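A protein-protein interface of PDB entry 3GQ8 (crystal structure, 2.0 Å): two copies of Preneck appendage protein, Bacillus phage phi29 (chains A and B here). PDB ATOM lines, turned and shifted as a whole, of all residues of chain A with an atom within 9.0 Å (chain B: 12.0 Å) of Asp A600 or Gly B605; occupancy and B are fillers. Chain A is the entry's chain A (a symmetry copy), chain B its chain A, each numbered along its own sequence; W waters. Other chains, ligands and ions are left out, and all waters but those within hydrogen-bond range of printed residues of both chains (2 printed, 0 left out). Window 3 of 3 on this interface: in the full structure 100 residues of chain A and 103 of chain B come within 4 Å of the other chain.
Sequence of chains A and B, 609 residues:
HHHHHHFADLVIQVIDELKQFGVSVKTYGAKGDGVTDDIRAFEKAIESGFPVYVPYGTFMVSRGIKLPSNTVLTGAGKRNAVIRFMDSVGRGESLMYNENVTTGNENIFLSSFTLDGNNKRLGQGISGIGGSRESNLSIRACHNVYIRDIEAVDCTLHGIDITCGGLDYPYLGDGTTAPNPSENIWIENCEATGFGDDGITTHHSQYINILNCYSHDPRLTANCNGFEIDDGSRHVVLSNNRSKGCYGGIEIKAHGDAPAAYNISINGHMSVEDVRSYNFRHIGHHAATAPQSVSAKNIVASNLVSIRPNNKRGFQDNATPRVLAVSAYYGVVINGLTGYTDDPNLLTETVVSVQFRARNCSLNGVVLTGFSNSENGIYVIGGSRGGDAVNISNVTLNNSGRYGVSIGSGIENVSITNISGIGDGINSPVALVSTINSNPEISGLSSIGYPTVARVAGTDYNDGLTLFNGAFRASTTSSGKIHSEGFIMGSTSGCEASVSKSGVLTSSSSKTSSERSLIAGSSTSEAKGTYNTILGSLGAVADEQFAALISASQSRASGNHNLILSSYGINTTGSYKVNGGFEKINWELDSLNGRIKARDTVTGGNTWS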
ATOM      1  N   ILE A 585      -1.405  31.987   5.362  1.00  0.00           N
ATOM      2  CA  ILE A 585      -2.769  32.499   5.579  1.00  0.00           C
ATOM      3  C   ILE A 585      -3.609  31.392   6.234  1.00  0.00           C
ATOM      4  O   ILE A 585      -3.600  30.245   5.765  1.00  0.00           O
ATOM      5  CB  ILE A 585      -3.422  32.955   4.265  1.00  0.00           C
ATOM      6  CG1 ILE A 585      -2.582  34.075   3.626  1.00  0.00           C
ATOM      7  CG2 ILE A 585      -4.897  33.386   4.510  1.00  0.00           C
ATOM      8  CD1 ILE A 585      -2.886  34.327   2.150  1.00  0.00           C
ATOM      9  N   ASN A 586      -4.327  31.734   7.309  1.00  0.00           N
ATOM     10  CA  ASN A 586      -5.087  30.754   8.098  1.00  0.00           C
ATOM     11  C   ASN A 586      -6.602  30.986   8.205  1.00  0.00           C
ATOM     12  O   ASN A 586      -7.349  30.055   8.519  1.00  0.00           O
ATOM     13  CB  ASN A 586      -4.471  30.599   9.495  1.00  0.00           C
ATOM     14  CG  ASN A 586      -3.145  29.838   9.471  1.00  0.00           C
ATOM     15  OD1 ASN A 586      -2.275  30.019  10.337  1.00  0.00           O
ATOM     16  ND2 ASN A 586      -2.984  28.996   8.483  1.00  0.00           N
ATOM     17  N   TRP A 587      -7.052  32.213   7.933  1.00  0.00           N
ATOM     18  CA  TRP A 587      -8.482  32.473   7.775  1.00  0.00           C
ATOM     19  C   TRP A 587      -8.760  33.616   6.829  1.00  0.00           C
ATOM     20  O   TRP A 587      -7.889  34.455   6.550  1.00  0.00           O
ATOM     21  CB  TRP A 587      -9.212  32.690   9.125  1.00  0.00           C
ATOM     22  CG  TRP A 587      -8.629  33.780   9.963  1.00  0.00           C
ATOM     23  CD1 TRP A 587      -7.744  33.637  11.003  1.00  0.00           C
ATOM     24  CD2 TRP A 587      -8.892  35.178   9.849  1.00  0.00           C
ATOM     25  NE1 TRP A 587      -7.432  34.869  11.528  1.00  0.00           N
ATOM     26  CE2 TRP A 587      -8.131  35.831  10.844  1.00  0.00           C
ATOM     27  CE3 TRP A 587      -9.690  35.948   8.992  1.00  0.00           C
ATOM     28  CZ2 TRP A 587      -8.137  37.222  11.001  1.00  0.00           C
ATOM     29  CZ3 TRP A 587      -9.699  37.336   9.151  1.00  0.00           C
ATOM     30  CH2 TRP A 587      -8.935  37.954  10.152  1.00  0.00           C
ATOM     31  N   ILE A 596     -16.515  32.439   4.084  1.00  0.00           N
ATOM     32  CA  ILE A 596     -15.660  32.452   5.267  1.00  0.00           C
ATOM     33  C   ILE A 596     -14.891  31.152   5.206  1.00  0.00           C
ATOM     34  O   ILE A 596     -15.483  30.093   4.981  1.00  0.00           O
ATOM     35  CB  ILE A 596     -16.480  32.584   6.571  1.00  0.00           C
ATOM     36  CG1 ILE A 596     -17.139  33.972   6.651  1.00  0.00           C
ATOM     37  CG2 ILE A 596     -15.596  32.332   7.812  1.00  0.00           C
ATOM     38  CD1 ILE A 596     -18.242  34.049   7.701  1.00  0.00           C
ATOM     39  N   LYS A 597     -13.572  31.239   5.359  1.00  0.00           N
ATOM     40  CA  LYS A 597     -12.689  30.092   5.191  1.00  0.00           C
ATOM     41  C   LYS A 597     -11.689  30.016   6.336  1.00  0.00           C
ATOM     42  O   LYS A 597     -11.123  31.030   6.733  1.00  0.00           O
ATOM     43  CB  LYS A 597     -11.909  30.211   3.878  1.00  0.00           C
ATOM     44  CG  LYS A 597     -12.769  30.286   2.618  1.00  0.00           C
ATOM     45  CD  LYS A 597     -11.890  30.592   1.415  1.00  0.00           C
ATOM     46  CE  LYS A 597     -12.487  30.067   0.129  1.00  0.00           C
ATOM     47  NZ  LYS A 597     -11.418  30.078  -0.933  1.00  0.00           N
ATOM     48  N   ALA A 598     -11.489  28.816   6.864  1.00  0.00           N
ATOM     49  CA  ALA A 598     -10.429  28.556   7.820  1.00  0.00           C
ATOM     50  C   ALA A 598      -9.513  27.485   7.224  1.00  0.00           C
ATOM     51  O   ALA A 598      -9.970  26.621   6.455  1.00  0.00           O
ATOM     52  CB  ALA A 598     -11.010  28.073   9.135  1.00  0.00           C
ATOM     53  N   ARG A 599      -8.231  27.534   7.562  1.00  0.00           N
ATOM     54  CA  ARG A 599      -7.319  26.441   7.172  1.00  0.00           C
ATOM     55  C   ARG A 599      -7.671  25.156   7.930  1.00  0.00           C
ATOM     56  O   ARG A 599      -7.623  24.069   7.370  1.00  0.00           O
ATOM     57  CB  ARG A 599      -5.867  26.812   7.455  1.00  0.00           C
ATOM     58  CG  ARG A 599      -4.865  25.732   7.045  1.00  0.00           C
ATOM     59  CD  ARG A 599      -3.430  26.213   7.136  1.00  0.00           C
ATOM     60  NE  ARG A 599      -3.145  27.285   6.188  1.00  0.00           N
ATOM     61  CZ  ARG A 599      -2.767  27.092   4.930  1.00  0.00           C
ATOM     62  NH1 ARG A 599      -2.631  25.854   4.452  1.00  0.00           N
ATOM     63  NH2 ARG A 599      -2.536  28.134   4.148  1.00  0.00           N
ATOM     64  N   ASP A 600      -7.987  25.284   9.214  1.00  0.00           N
ATOM     65  CA  ASP A 600      -8.339  24.120  10.028  1.00  0.00           C
ATOM     66  C   ASP A 600      -9.870  24.019  10.144  1.00  0.00           C
ATOM     67  O   ASP A 600     -10.541  23.791   9.136  1.00  0.00           O
ATOM     68  CB  ASP A 600      -7.601  24.149  11.384  1.00  0.00           C
ATOM     69  CG  ASP A 600      -7.730  22.842  12.164  1.00  0.00           C
ATOM     70  OD1 ASP A 600      -7.682  21.757  11.550  1.00  0.00           O
ATOM     71  OD2 ASP A 600      -7.895  22.902  13.405  1.00  0.00           O
ATOM     72  N   THR A 601     -10.431  24.199  11.334  1.00  0.00           N
ATOM     73  CA  THR A 601     -11.870  23.958  11.523  1.00  0.00           C
ATOM     74  C   THR A 601     -12.689  25.237  11.682  1.00  0.00           C
ATOM     75  O   THR A 601     -12.164  26.276  12.080  1.00  0.00           O
ATOM     76  CB  THR A 601     -12.130  23.095  12.765  1.00  0.00           C
ATOM     77  OG1 THR A 601     -11.565  23.745  13.908  1.00  0.00           O
ATOM     78  CG2 THR A 601     -11.514  21.689  12.609  1.00  0.00           C
ATOM     79  N   VAL A 602     -13.977  25.149  11.359  1.00  0.00           N
ATOM     80  CA  VAL A 602     -14.936  26.188  11.693  1.00  0.00           C
ATOM     81  C   VAL A 602     -16.015  25.514  12.525  1.00  0.00           C
ATOM     82  O   VAL A 602     -16.605  24.528  12.074  1.00  0.00           O
ATOM     83  CB  VAL A 602     -15.602  26.809  10.453  1.00  0.00           C
ATOM     84  CG1 VAL A 602     -16.486  27.956  10.883  1.00  0.00           C
ATOM     85  CG2 VAL A 602     -14.569  27.324   9.461  1.00  0.00           C
ATOM     86  N   THR A 603     -16.274  26.017  13.734  1.00  0.00           N
ATOM     87  CA  THR A 603     -17.206  25.338  14.637  1.00  0.00           C
ATOM     88  C   THR A 603     -18.066  26.308  15.433  1.00  0.00           C
ATOM     89  O   THR A 603     -17.633  27.418  15.744  1.00  0.00           O
ATOM     90  CB  THR A 603     -16.478  24.421  15.647  1.00  0.00           C
ATOM     91  OG1 THR A 603     -15.478  25.174  16.336  1.00  0.00           O
ATOM     92  CG2 THR A 603     -15.820  23.219  14.952  1.00  0.00           C
ATOM     93  N   THR B 601     -20.715  30.244   1.449  1.00  0.00           N
ATOM     94  CA  THR B 601     -20.296  29.080   2.244  1.00  0.00           C
ATOM     95  C   THR B 601     -19.391  29.438   3.421  1.00  0.00           C
ATOM     96  O   THR B 601     -18.724  30.472   3.413  1.00  0.00           O
ATOM     97  CB  THR B 601     -19.537  28.063   1.382  1.00  0.00           C
ATOM     98  OG1 THR B 601     -18.408  28.710   0.785  1.00  0.00           O
ATOM     99  CG2 THR B 601     -20.442  27.477   0.279  1.00  0.00           C
ATOM    100  N   VAL B 602     -19.384  28.576   4.434  1.00  0.00           N
ATOM    101  CA  VAL B 602     -18.398  28.636   5.500  1.00  0.00           C
ATOM    102  C   VAL B 602     -17.703  27.283   5.509  1.00  0.00           C
ATOM    103  O   VAL B 602     -18.375  26.254   5.617  1.00  0.00           O
ATOM    104  CB  VAL B 602     -19.027  28.862   6.886  1.00  0.00           C
ATOM    105  CG1 VAL B 602     -17.931  29.033   7.910  1.00  0.00           C
ATOM    106  CG2 VAL B 602     -19.917  30.095   6.902  1.00  0.00           C
ATOM    107  N   THR B 603     -16.374  27.265   5.383  1.00  0.00           N
ATOM    108  CA  THR B 603     -15.658  25.994   5.252  1.00  0.00           C
ATOM    109  C   THR B 603     -14.329  25.989   5.992  1.00  0.00           C
ATOM    110  O   THR B 603     -13.683  27.029   6.127  1.00  0.00           O
ATOM    111  CB  THR B 603     -15.372  25.634   3.776  1.00  0.00           C
ATOM    112  OG1 THR B 603     -14.700  26.725   3.143  1.00  0.00           O
ATOM    113  CG2 THR B 603     -16.665  25.320   3.007  1.00  0.00           C
ATOM    114  N   GLY B 604     -13.933  24.805   6.457  1.00  0.00           N
ATOM    115  CA  GLY B 604     -12.589  24.574   6.968  1.00  0.00           C
ATOM    116  C   GLY B 604     -11.775  23.810   5.937  1.00  0.00           C
ATOM    117  O   GLY B 604     -12.259  23.548   4.832  1.00  0.00           O
ATOM    118  N   GLY B 605     -10.540  23.460   6.283  1.00  0.00           N
ATOM    119  CA  GLY B 605      -9.681  22.660   5.391  1.00  0.00           C
ATOM    120  C   GLY B 605      -9.210  23.355   4.121  1.00  0.00           C
ATOM    121  O   GLY B 605      -8.913  22.703   3.110  1.00  0.00           O
ATOM    122  N   ASN B 606      -9.120  24.681   4.168  1.00  0.00           N
ATOM    123  CA  ASN B 606      -8.712  25.470   3.016  1.00  0.00           C
ATOM    124  C   ASN B 606      -7.209  25.675   2.928  1.00  0.00           C
ATOM    125  O   ASN B 606      -6.516  25.683   3.945  1.00  0.00           O
ATOM    126  CB  ASN B 606      -9.380  26.847   3.082  1.00  0.00           C
ATOM    127  CG  ASN B 606     -10.849  26.783   2.793  1.00  0.00           C
ATOM    128  OD1 ASN B 606     -11.252  26.661   1.639  1.00  0.00           O
ATOM    129  ND2 ASN B 606     -11.666  26.858   3.835  1.00  0.00           N
ATOM    130  N   THR B 607      -6.711  25.874   1.709  1.00  0.00           N
ATOM    131  CA  THR B 607      -5.357  26.402   1.523  1.00  0.00           C
ATOM    132  C   THR B 607      -5.403  27.614   0.593  1.00  0.00           C
ATOM    133  O   THR B 607      -6.392  27.822  -0.113  1.00  0.00           O
ATOM    134  CB  THR B 607      -4.329  25.320   1.032  1.00  0.00           C
ATOM    135  OG1 THR B 607      -2.990  25.735   1.367  1.00  0.00           O
ATOM    136  CG2 THR B 607      -4.429  25.097  -0.490  1.00  0.00           C
ATOM    137  N   TRP B 608      -4.350  28.422   0.606  1.00  0.00           N
ATOM    138  CA  TRP B 608      -4.334  29.642  -0.187  1.00  0.00           C
ATOM    139  C   TRP B 608      -3.363  29.603  -1.382  1.00  0.00           C
ATOM    140  O   TRP B 608      -2.504  30.471  -1.548  1.00  0.00           O
ATOM    141  CB  TRP B 608      -4.125  30.861   0.712  1.00  0.00           C
ATOM    142  CG  TRP B 608      -5.415  31.304   1.378  1.00  0.00           C
ATOM    143  CD1 TRP B 608      -6.196  32.374   1.022  1.00  0.00           C
ATOM    144  CD2 TRP B 608      -6.072  30.683   2.500  1.00  0.00           C
ATOM    145  NE1 TRP B 608      -7.287  32.462   1.860  1.00  0.00           N
ATOM    146  CE2 TRP B 608      -7.242  31.437   2.768  1.00  0.00           C
ATOM    147  CE3 TRP B 608      -5.782  29.576   3.311  1.00  0.00           C
ATOM    148  CZ2 TRP B 608      -8.118  31.116   3.806  1.00  0.00           C
ATOM    149  CZ3 TRP B 608      -6.673  29.252   4.350  1.00  0.00           C
ATOM    150  CH2 TRP B 608      -7.821  30.024   4.583  1.00  0.00           C
ATOM    151  N   SER B 609      -3.532  28.574  -2.204  1.00  0.00           N
ATOM    152  CA  SER B 609      -2.771  28.391  -3.446  1.00  0.00           C
ATOM    153  C   SER B 609      -3.493  27.394  -4.339  1.00  0.00           C
ATOM    154  O   SER B 609      -4.299  26.586  -3.854  1.00  0.00           O
ATOM    155  CB  SER B 609      -1.371  27.859  -3.158  1.00  0.00           C
ATOM    156  OG  SER B 609      -1.434  26.604  -2.502  1.00  0.00           O
ATOM    157  OXT SER B 609      -3.259  27.360  -5.553  1.00  0.00           O
HETATM  158  O   HOH W   1      -6.029  23.016   5.205  1.00  0.00           O
HETATM  159  O   HOH W   2     -16.170  28.909   2.320  1.00  0.00           O
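Asp A600 touches two residues of chain B. Of the printed residues of chain A, Gly B605 touches Ala A598 (3.2 Å), Arg A599 (3.2 Å) and Asp A600 (2.9 Å). Printed residues of chain B within 4 Å of Asn A586: Trp B608 (3.9 Å). Of chain B, only Thr B603, Gly B604, Gly B605 and Asn B606 come within 4 Å of Ala A598. Gly B604 touches just these residues of chain A: Ala A598 (3.4 Å), Asp A600 (3.1 Å) and Val A602 (3.97 Å). Asn B606 touches three residues of chain A. Printed residues of chain A within 4 Å of Val B602: Ile A596 and Val A602. Of the printed residues of chain B, Trp A587 touches Trp B608. Thr A603 touches none of the printed residues of chain B. The nearest residue of chain B that does not touch Asp A600 is Asn B606 (5.2 Å). The nearest residue of chain A that does not touch Gly B605 is Thr A601 (5.1 Å).
Val B602 touches its own counterpart, Val A602. Val A602 touches Thr B603, but with the chains exchanged Thr A603 does not touch Val B602 (6.8 Å). Positions printed for both chains: 601, 602 and 603.
Of the 11 printed residues of chain A, 9 touch a printed residue of chain B. Hydrophobic or aromatic side chains of chain A within 4 Å of the printed part of chain B: Ile A585 and Val A602. Of the 9 printed residues of chain B, 8 touch a printed residue of chain A. Hydrophobic or aromatic side chains of chain B that line the printed part of chain A: Val B602 and Trp B608. Among the printed residues, no Asp or Glu carboxylate lies within 4 Å of a Lys or Arg side-chain nitrogen of the other chain.
Among the printed residues, pairs that only touch across the chains: Asp A600 with Gly B604, Ile A596 with Val B602, Ile A585 with Trp B608, Lys A597 with Thr B603, Lys A597 with Asn B606, Ala A598 with Gly B604, Arg A599 with Asn B606, Val A602 with Thr B603, Val A602 with Val B602, Arg A599 with Trp B608, Lys A597 with Trp B608, Asn A586 with Trp B608, Val A602 with Gly B604 and Trp A587 with Trp B608.
Water W2 lies within hydrogen-bond range of OG1 of Thr B601, OG1 of Thr B603 and O of Ile A596. Water W1 lies within hydrogen-bond range of the backbone carbonyl oxygen (O) of Arg A599 (2.9 Å) and the backbone carbonyl oxygen (O) of Asn B606 (3.0 Å).
The backbone NH of Gly B605 sits at hydrogen-bond distance from the backbone carbonyl oxygen of Ala A598 (3.2 Å). The backbone carbonyl oxygen of Asp A600 is in hydrogen-bond range of the backbone NH of Gly B605. The backbone NH of Ala A598 sits at hydrogen-bond distance from the backbone carbonyl oxygen of Thr B603 (2.9 Å). The side-chain hydroxyl (OG1) of Thr B607 lies within hydrogen-bond range of the guanidinium group (NH1) of Arg A599. The backbone carbonyl oxygen of Ile A596 lies within hydrogen-bond range of the backbone NH of Thr B603 (3.0 Å). The backbone NH of Asn B606 is in hydrogen-bond range of the backbone carbonyl oxygen of Ala A598 (3.1 Å). The backbone carbonyl oxygen (O) of Thr B601 is in hydrogen-bond range of the backbone NH (N) of Ile A596, 3.0 Å away. N of Gly B605 lies within hydrogen-bond range of O of Arg A599, at 3.2 Å.
O of Thr B603 sits at hydrogen-bond distance from ND2 of Asn B606, 3.1 Å away. The backbone NH (N) of Arg A599 lies within hydrogen-bond range of the backbone carbonyl oxygen (O) of Asn A586, 2.8 Å away. The guanidinium group (NH2) of Arg A599 is in hydrogen-bond range of the backbone carbonyl oxygen (O) of Ile A585, 2.9 Å away.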
